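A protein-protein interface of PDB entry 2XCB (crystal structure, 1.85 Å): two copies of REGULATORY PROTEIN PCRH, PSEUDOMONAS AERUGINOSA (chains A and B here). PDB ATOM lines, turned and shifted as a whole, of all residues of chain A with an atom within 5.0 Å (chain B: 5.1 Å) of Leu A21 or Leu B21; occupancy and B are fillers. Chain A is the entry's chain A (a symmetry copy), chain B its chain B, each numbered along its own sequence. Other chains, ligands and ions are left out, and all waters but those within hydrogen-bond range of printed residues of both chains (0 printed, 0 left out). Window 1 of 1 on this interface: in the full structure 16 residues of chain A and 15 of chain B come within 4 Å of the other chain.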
ATOM      1  N   LEU A  13       6.501 -19.259 -24.118  1.00  0.00           N
ATOM      2  CA  LEU A  13       6.100 -17.959 -23.518  1.00  0.00           C
ATOM      3  C   LEU A  13       6.479 -17.799 -22.031  1.00  0.00           C
ATOM      4  O   LEU A  13       6.472 -18.770 -21.262  1.00  0.00           O
ATOM      5  CB  LEU A  13       4.601 -17.702 -23.679  1.00  0.00           C
ATOM      6  CG  LEU A  13       3.900 -17.585 -25.040  1.00  0.00           C
ATOM      7  CD1 LEU A  13       2.351 -17.562 -24.834  1.00  0.00           C
ATOM      8  CD2 LEU A  13       4.368 -16.379 -25.897  1.00  0.00           C
ATOM      9  N   THR A  17       3.441 -13.623 -19.420  1.00  0.00           N
ATOM     10  CA  THR A  17       2.509 -13.683 -20.578  1.00  0.00           C
ATOM     11  C   THR A  17       1.447 -14.768 -20.400  1.00  0.00           C
ATOM     12  O   THR A  17       0.275 -14.503 -20.656  1.00  0.00           O
ATOM     13  CB  THR A  17       3.215 -13.884 -21.959  1.00  0.00           C
ATOM     14  OG1 THR A  17       4.069 -12.769 -22.190  1.00  0.00           O
ATOM     15  CG2 THR A  17       2.179 -13.917 -23.137  1.00  0.00           C
ATOM     16  N   LEU A  18       1.846 -15.973 -19.969  1.00  0.00           N
ATOM     17  CA  LEU A  18       0.824 -16.981 -19.535  1.00  0.00           C
ATOM     18  C   LEU A  18      -0.209 -16.469 -18.542  1.00  0.00           C
ATOM     19  O   LEU A  18      -1.398 -16.708 -18.684  1.00  0.00           O
ATOM     20  CB  LEU A  18       1.480 -18.240 -18.984  1.00  0.00           C
ATOM     21  CG  LEU A  18       2.293 -18.935 -20.053  1.00  0.00           C
ATOM     22  CD1 LEU A  18       3.173 -19.987 -19.466  1.00  0.00           C
ATOM     23  CD2 LEU A  18       1.387 -19.492 -21.118  1.00  0.00           C
ATOM     24  N   GLU A  19       0.238 -15.722 -17.540  1.00  0.00           N
ATOM     25  CA  GLU A  19      -0.651 -15.128 -16.567  1.00  0.00           C
ATOM     26  C   GLU A  19      -1.653 -14.179 -17.202  1.00  0.00           C
ATOM     27  O   GLU A  19      -2.850 -14.188 -16.873  1.00  0.00           O
ATOM     28  CB  GLU A  19       0.153 -14.416 -15.490  1.00  0.00           C
ATOM     29  CG  GLU A  19      -0.609 -14.203 -14.181  1.00  0.00           C
ATOM     30  CD  GLU A  19      -1.525 -15.405 -13.761  1.00  0.00           C
ATOM     31  OE1 GLU A  19      -1.000 -16.551 -13.666  1.00  0.00           O
ATOM     32  OE2 GLU A  19      -2.766 -15.148 -13.558  1.00  0.00           O
ATOM     33  N   GLN A  20      -1.191 -13.364 -18.135  1.00  0.00           N
ATOM     34  CA  GLN A  20      -2.118 -12.487 -18.842  1.00  0.00           C
ATOM     35  C   GLN A  20      -3.066 -13.238 -19.769  1.00  0.00           C
ATOM     36  O   GLN A  20      -4.253 -12.855 -19.954  1.00  0.00           O
ATOM     37  CB  GLN A  20      -1.339 -11.401 -19.607  1.00  0.00           C
ATOM     38  CG  GLN A  20      -0.603 -10.428 -18.681  1.00  0.00           C
ATOM     39  CD  GLN A  20       0.390  -9.545 -19.458  1.00  0.00           C
ATOM     40  OE1 GLN A  20       0.074  -9.080 -20.545  1.00  0.00           O
ATOM     41  NE2 GLN A  20       1.595  -9.337 -18.907  1.00  0.00           N
ATOM     42  N   LEU A  21      -2.583 -14.333 -20.323  1.00  0.00           N
ATOM     43  CA  LEU A  21      -3.442 -15.157 -21.156  1.00  0.00           C
ATOM     44  C   LEU A  21      -4.490 -15.909 -20.316  1.00  0.00           C
ATOM     45  O   LEU A  21      -5.636 -16.064 -20.742  1.00  0.00           O
ATOM     46  CB  LEU A  21      -2.545 -16.144 -21.834  1.00  0.00           C
ATOM     47  CG  LEU A  21      -2.694 -16.472 -23.292  1.00  0.00           C
ATOM     48  CD1 LEU A  21      -3.261 -15.258 -24.046  1.00  0.00           C
ATOM     49  CD2 LEU A  21      -1.317 -16.903 -23.810  1.00  0.00           C
ATOM     50  N   TYR A  22      -4.095 -16.369 -19.123  1.00  0.00           N
ATOM     51  CA  TYR A  22      -5.076 -16.916 -18.198  1.00  0.00           C
ATOM     52  C   TYR A  22      -6.120 -15.899 -17.819  1.00  0.00           C
ATOM     53  O   TYR A  22      -7.324 -16.210 -17.849  1.00  0.00           O
ATOM     54  CB  TYR A  22      -4.415 -17.588 -16.986  1.00  0.00           C
ATOM     55  CG  TYR A  22      -5.445 -17.988 -15.914  1.00  0.00           C
ATOM     56  CD1 TYR A  22      -6.176 -19.154 -16.045  1.00  0.00           C
ATOM     57  CD2 TYR A  22      -5.751 -17.132 -14.830  1.00  0.00           C
ATOM     58  CE1 TYR A  22      -7.118 -19.530 -15.094  1.00  0.00           C
ATOM     59  CE2 TYR A  22      -6.746 -17.503 -13.866  1.00  0.00           C
ATOM     60  CZ  TYR A  22      -7.411 -18.661 -14.030  1.00  0.00           C
ATOM     61  OH  TYR A  22      -8.336 -19.031 -13.114  1.00  0.00           O
ATOM     62  N   ALA A  23      -5.697 -14.658 -17.484  1.00  0.00           N
ATOM     63  CA  ALA A  23      -6.627 -13.555 -17.266  1.00  0.00           C
ATOM     64  C   ALA A  23      -7.611 -13.336 -18.398  1.00  0.00           C
ATOM     65  O   ALA A  23      -8.809 -12.999 -18.166  1.00  0.00           O
ATOM     66  CB  ALA A  23      -5.858 -12.211 -17.022  1.00  0.00           C
ATOM     67  N   LEU A  24      -7.100 -13.445 -19.621  1.00  0.00           N
ATOM     68  CA  LEU A  24      -7.913 -13.186 -20.810  1.00  0.00           C
ATOM     69  C   LEU A  24      -8.995 -14.253 -20.867  1.00  0.00           C
ATOM     70  O   LEU A  24     -10.188 -13.933 -21.032  1.00  0.00           O
ATOM     71  CB  LEU A  24      -7.047 -13.140 -22.096  1.00  0.00           C
ATOM     72  CG  LEU A  24      -7.654 -12.785 -23.463  1.00  0.00           C
ATOM     73  CD1 LEU A  24      -6.629 -12.084 -24.324  1.00  0.00           C
ATOM     74  CD2 LEU A  24      -8.053 -14.012 -24.203  1.00  0.00           C
ATOM     75  N   GLY A  25      -8.578 -15.505 -20.666  1.00  0.00           N
ATOM     76  CA  GLY A  25      -9.482 -16.651 -20.680  1.00  0.00           C
ATOM     77  C   GLY A  25     -10.492 -16.592 -19.580  1.00  0.00           C
ATOM     78  O   GLY A  25     -11.646 -16.832 -19.815  1.00  0.00           O
ATOM     79  N   ILE A  40      -8.941 -20.487 -25.434  1.00  0.00           N
ATOM     80  CA  ILE A  40      -7.815 -19.976 -24.647  1.00  0.00           C
ATOM     81  C   ILE A  40      -7.301 -21.015 -23.602  1.00  0.00           C
ATOM     82  O   ILE A  40      -6.088 -21.290 -23.481  1.00  0.00           O
ATOM     83  CB  ILE A  40      -8.247 -18.651 -24.016  1.00  0.00           C
ATOM     84  CG1 ILE A  40      -8.548 -17.676 -25.165  1.00  0.00           C
ATOM     85  CG2 ILE A  40      -7.180 -18.132 -23.023  1.00  0.00           C
ATOM     86  CD1 ILE A  40      -7.253 -17.151 -25.833  1.00  0.00           C
ATOM     87  N   LEU A  44      -3.658 -22.889 -23.182  1.00  0.00           N
ATOM     88  CA  LEU A  44      -2.879 -22.921 -21.985  1.00  0.00           C
ATOM     89  C   LEU A  44      -2.558 -24.339 -21.439  1.00  0.00           C
ATOM     90  O   LEU A  44      -1.404 -24.570 -21.069  1.00  0.00           O
ATOM     91  CB  LEU A  44      -3.516 -22.081 -20.910  1.00  0.00           C
ATOM     92  CG  LEU A  44      -3.509 -20.576 -21.163  1.00  0.00           C
ATOM     93  CD1 LEU A  44      -4.627 -20.043 -20.375  1.00  0.00           C
ATOM     94  CD2 LEU A  44      -2.139 -19.906 -20.753  1.00  0.00           C
ATOM     95  N   LEU A  47       0.345 -25.435 -23.432  1.00  0.00           N
ATOM     96  CA  LEU A  47       1.519 -24.702 -23.034  1.00  0.00           C
ATOM     97  C   LEU A  47       2.047 -25.073 -21.666  1.00  0.00           C
ATOM     98  O   LEU A  47       3.233 -24.916 -21.402  1.00  0.00           O
ATOM     99  CB  LEU A  47       1.149 -23.172 -22.983  1.00  0.00           C
ATOM    100  CG  LEU A  47       0.959 -22.556 -24.388  1.00  0.00           C
ATOM    101  CD1 LEU A  47       0.553 -21.133 -24.348  1.00  0.00           C
ATOM    102  CD2 LEU A  47       2.246 -22.772 -25.193  1.00  0.00           C
ATOM    103  N   LEU B  13     -11.651 -17.218 -33.130  1.00  0.00           N
ATOM    104  CA  LEU B  13     -11.972 -16.366 -32.002  1.00  0.00           C
ATOM    105  C   LEU B  13     -12.854 -15.189 -32.419  1.00  0.00           C
ATOM    106  O   LEU B  13     -12.806 -14.752 -33.570  1.00  0.00           O
ATOM    107  CB  LEU B  13     -10.700 -15.875 -31.300  1.00  0.00           C
ATOM    108  CG  LEU B  13      -9.869 -16.954 -30.586  1.00  0.00           C
ATOM    109  CD1 LEU B  13      -8.508 -16.391 -30.258  1.00  0.00           C
ATOM    110  CD2 LEU B  13     -10.619 -17.451 -29.302  1.00  0.00           C
ATOM    111  N   ASP B  16     -13.814  -9.428 -30.377  1.00  0.00           N
ATOM    112  CA  ASP B  16     -13.444  -8.844 -29.103  1.00  0.00           C
ATOM    113  C   ASP B  16     -12.224  -9.549 -28.493  1.00  0.00           C
ATOM    114  O   ASP B  16     -11.351  -8.912 -27.913  1.00  0.00           O
ATOM    115  CB  ASP B  16     -14.657  -8.933 -28.178  1.00  0.00           C
ATOM    116  CG  ASP B  16     -14.347  -8.529 -26.771  1.00  0.00           C
ATOM    117  OD1 ASP B  16     -13.821  -7.406 -26.553  1.00  0.00           O
ATOM    118  OD2 ASP B  16     -14.636  -9.351 -25.877  1.00  0.00           O
ATOM    119  N   THR B  17     -12.196 -10.879 -28.623  1.00  0.00           N
ATOM    120  CA  THR B  17     -11.104 -11.706 -28.058  1.00  0.00           C
ATOM    121  C   THR B  17      -9.801 -11.408 -28.820  1.00  0.00           C
ATOM    122  O   THR B  17      -8.787 -11.112 -28.202  1.00  0.00           O
ATOM    123  CB  THR B  17     -11.426 -13.235 -28.142  1.00  0.00           C
ATOM    124  OG1 THR B  17     -12.515 -13.560 -27.242  1.00  0.00           O
ATOM    125  CG2 THR B  17     -10.183 -14.066 -27.755  1.00  0.00           C
ATOM    126  N   LEU B  18      -9.870 -11.471 -30.163  1.00  0.00           N
ATOM    127  CA  LEU B  18      -8.745 -11.072 -31.061  1.00  0.00           C
ATOM    128  C   LEU B  18      -8.211  -9.722 -30.688  1.00  0.00           C
ATOM    129  O   LEU B  18      -7.006  -9.548 -30.534  1.00  0.00           O
ATOM    130  CB  LEU B  18      -9.153 -11.108 -32.513  1.00  0.00           C
ATOM    131  CG  LEU B  18      -9.277 -12.543 -32.984  1.00  0.00           C
ATOM    132  CD1 LEU B  18      -9.996 -12.613 -34.303  1.00  0.00           C
ATOM    133  CD2 LEU B  18      -7.887 -13.257 -33.047  1.00  0.00           C
ATOM    134  N   GLU B  19      -9.092  -8.754 -30.464  1.00  0.00           N
ATOM    135  CA  GLU B  19      -8.600  -7.418 -30.101  1.00  0.00           C
ATOM    136  C   GLU B  19      -7.867  -7.400 -28.763  1.00  0.00           C
ATOM    137  O   GLU B  19      -6.821  -6.748 -28.609  1.00  0.00           O
ATOM    138  CB  GLU B  19      -9.764  -6.434 -30.092  1.00  0.00           C
ATOM    139  CG  GLU B  19      -9.406  -4.983 -29.714  1.00  0.00           C
ATOM    140  CD  GLU B  19      -8.573  -4.270 -30.786  1.00  0.00           C
ATOM    141  OE1 GLU B  19      -8.656  -4.617 -31.993  1.00  0.00           O
ATOM    142  OE2 GLU B  19      -7.826  -3.364 -30.401  1.00  0.00           O
ATOM    143  N   GLN B  20      -8.417  -8.122 -27.775  1.00  0.00           N
ATOM    144  CA  GLN B  20      -7.782  -8.221 -26.456  1.00  0.00           C
ATOM    145  C   GLN B  20      -6.458  -8.949 -26.592  1.00  0.00           C
ATOM    146  O   GLN B  20      -5.480  -8.649 -25.903  1.00  0.00           O
ATOM    147  CB  GLN B  20      -8.729  -8.888 -25.427  1.00  0.00           C
ATOM    148  CG  GLN B  20     -10.153  -8.201 -25.332  1.00  0.00           C
ATOM    149  CD  GLN B  20     -11.118  -8.778 -24.231  1.00  0.00           C
ATOM    150  OE1 GLN B  20     -10.691  -9.164 -23.136  1.00  0.00           O
ATOM    151  NE2 GLN B  20     -12.414  -8.804 -24.538  1.00  0.00           N
ATOM    152  N   LEU B  21      -6.392  -9.904 -27.497  1.00  0.00           N
ATOM    153  CA  LEU B  21      -5.132 -10.634 -27.680  1.00  0.00           C
ATOM    154  C   LEU B  21      -4.097  -9.670 -28.303  1.00  0.00           C
ATOM    155  O   LEU B  21      -2.955  -9.576 -27.844  1.00  0.00           O
ATOM    156  CB  LEU B  21      -5.368 -11.806 -28.614  1.00  0.00           C
ATOM    157  CG  LEU B  21      -4.197 -12.794 -28.685  1.00  0.00           C
ATOM    158  CD1 LEU B  21      -3.942 -13.532 -27.339  1.00  0.00           C
ATOM    159  CD2 LEU B  21      -4.473 -13.791 -29.810  1.00  0.00           C
ATOM    160  N   TYR B  22      -4.540  -8.953 -29.346  1.00  0.00           N
ATOM    161  CA  TYR B  22      -3.719  -7.899 -29.947  1.00  0.00           C
ATOM    162  C   TYR B  22      -3.245  -6.952 -28.848  1.00  0.00           C
ATOM    163  O   TYR B  22      -2.064  -6.685 -28.746  1.00  0.00           O
ATOM    164  CB  TYR B  22      -4.428  -7.117 -31.087  1.00  0.00           C
ATOM    165  CG  TYR B  22      -3.617  -5.860 -31.386  1.00  0.00           C
ATOM    166  CD1 TYR B  22      -2.354  -5.961 -31.984  1.00  0.00           C
ATOM    167  CD2 TYR B  22      -4.072  -4.597 -31.002  1.00  0.00           C
ATOM    168  CE1 TYR B  22      -1.594  -4.844 -32.212  1.00  0.00           C
ATOM    169  CE2 TYR B  22      -3.304  -3.469 -31.234  1.00  0.00           C
ATOM    170  CZ  TYR B  22      -2.079  -3.609 -31.833  1.00  0.00           C
ATOM    171  OH  TYR B  22      -1.302  -2.516 -32.055  1.00  0.00           O
ATOM    172  N   ALA B  23      -4.150  -6.471 -27.990  1.00  0.00           N
ATOM    173  CA  ALA B  23      -3.702  -5.519 -26.938  1.00  0.00           C
ATOM    174  C   ALA B  23      -2.710  -6.104 -25.939  1.00  0.00           C
ATOM    175  O   ALA B  23      -1.819  -5.400 -25.427  1.00  0.00           O
ATOM    176  CB  ALA B  23      -4.886  -4.906 -26.221  1.00  0.00           C
ATOM    177  N   LEU B  24      -2.832  -7.396 -25.655  1.00  0.00           N
ATOM    178  CA  LEU B  24      -1.789  -8.072 -24.854  1.00  0.00           C
ATOM    179  C   LEU B  24      -0.416  -8.110 -25.556  1.00  0.00           C
ATOM    180  O   LEU B  24       0.608  -7.883 -24.910  1.00  0.00           O
ATOM    181  CB  LEU B  24      -2.239  -9.501 -24.448  1.00  0.00           C
ATOM    182  CG  LEU B  24      -1.448 -10.569 -23.686  1.00  0.00           C
ATOM    183  CD1 LEU B  24      -2.303 -11.894 -23.532  1.00  0.00           C
ATOM    184  CD2 LEU B  24      -0.132 -10.931 -24.349  1.00  0.00           C
ATOM    185  N   GLY B  25      -0.389  -8.475 -26.847  1.00  0.00           N
ATOM    186  CA  GLY B  25       0.849  -8.381 -27.638  1.00  0.00           C
ATOM    187  C   GLY B  25       1.507  -7.003 -27.567  1.00  0.00           C
ATOM    188  O   GLY B  25       2.697  -6.861 -27.298  1.00  0.00           O
ATOM    189  N   ILE B  40       3.018 -13.620 -30.133  1.00  0.00           N
ATOM    190  CA  ILE B  40       1.643 -13.222 -30.144  1.00  0.00           C
ATOM    191  C   ILE B  40       1.252 -12.614 -31.519  1.00  0.00           C
ATOM    192  O   ILE B  40       0.185 -12.901 -32.051  1.00  0.00           O
ATOM    193  CB  ILE B  40       1.306 -12.208 -29.038  1.00  0.00           C
ATOM    194  CG1 ILE B  40       1.669 -12.769 -27.638  1.00  0.00           C
ATOM    195  CG2 ILE B  40      -0.165 -11.858 -29.095  1.00  0.00           C
ATOM    196  CD1 ILE B  40       0.874 -13.935 -27.255  1.00  0.00           C
ATOM    197  N   LEU B  44      -1.535 -13.727 -34.360  1.00  0.00           N
ATOM    198  CA  LEU B  44      -2.521 -12.823 -34.926  1.00  0.00           C
ATOM    199  C   LEU B  44      -2.461 -12.700 -36.464  1.00  0.00           C
ATOM    200  O   LEU B  44      -3.514 -12.726 -37.137  1.00  0.00           O
ATOM    201  CB  LEU B  44      -2.427 -11.461 -34.248  1.00  0.00           C
ATOM    202  CG  LEU B  44      -2.949 -11.481 -32.809  1.00  0.00           C
ATOM    203  CD1 LEU B  44      -2.464 -10.237 -32.023  1.00  0.00           C
ATOM    204  CD2 LEU B  44      -4.493 -11.524 -32.792  1.00  0.00           C
ATOM    205  N   LEU B  47      -4.007 -16.078 -37.700  1.00  0.00           N
ATOM    206  CA  LEU B  47      -5.367 -16.464 -37.280  1.00  0.00           C
ATOM    207  C   LEU B  47      -6.423 -15.484 -37.779  1.00  0.00           C
ATOM    208  O   LEU B  47      -7.546 -15.876 -38.131  1.00  0.00           O
ATOM    209  CB  LEU B  47      -5.483 -16.485 -35.759  1.00  0.00           C
ATOM    210  CG  LEU B  47      -4.571 -17.324 -34.856  1.00  0.00           C
ATOM    211  CD1 LEU B  47      -4.774 -16.964 -33.388  1.00  0.00           C
ATOM    212  CD2 LEU B  47      -4.807 -18.824 -35.095  1.00  0.00           C
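Among the printed residues, pairs that only touch across the chains: Leu A21 with Leu B24 (3.5 Å), Leu A21 with Leu B21 (3.8 Å), Gln A20 with Leu B24 (3.8 Å), Leu A24 with Leu B21 (3.9 Å), Leu A24 with Gln B20 (3.9 Å) and Thr A17 with Leu B24 (3.97 Å).
NE2 of Gln B20 is in hydrogen-bond range of OD2 of Asp B16, 2.7 Å away.
Thr A17 touches Leu B24, but with the chains exchanged Leu A24 does not touch Thr B17 (4.1 Å).
Gln A20 touches Leu B24, and with the chains exchanged Leu A24 touches Gln B20.
Leu B21 touches its own counterpart, Leu A21.
Leu A21 touches Leu B24, and with the chains exchanged Leu A24 touches Leu B21.
Of the 6 pairs that touch across the chains among the printed residues, 5 have their exchanged pair printed and touching as well.
Of the 14 printed residues of chain B, 3 touch a printed residue of chain A.
Of the 13 printed residues of chain A, 4 touch a printed residue of chain B.
Hydrophobic or aromatic side chains of chain A that line the printed part of chain B: Leu A21 and Leu A24.
Among the printed residues, 6 pairs touch across the chains.
Among the printed residues, no Asp or Glu carboxylate lies within 4 Å of a Lys or Arg side-chain nitrogen of the other chain.
Leu A21 touches just these residues of chain B: Leu B21 (3.8 Å) and Leu B24 (3.5 Å).
Of chain A, only Leu A21 and Leu A24 come within 4 Å of Leu B21.
Printed residues of chain B within 4 Å of Gln A20: Leu B24 (3.8 Å).
Printed residues of chain B within 4 Å of Thr A17: Leu B24.
The nearest printed residue of chain A that does not touch Leu B21 is Ile A40 (5.1 Å).
The nearest printed residue of chain A that does not touch Leu B24 is Leu A24 (4.4 Å).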
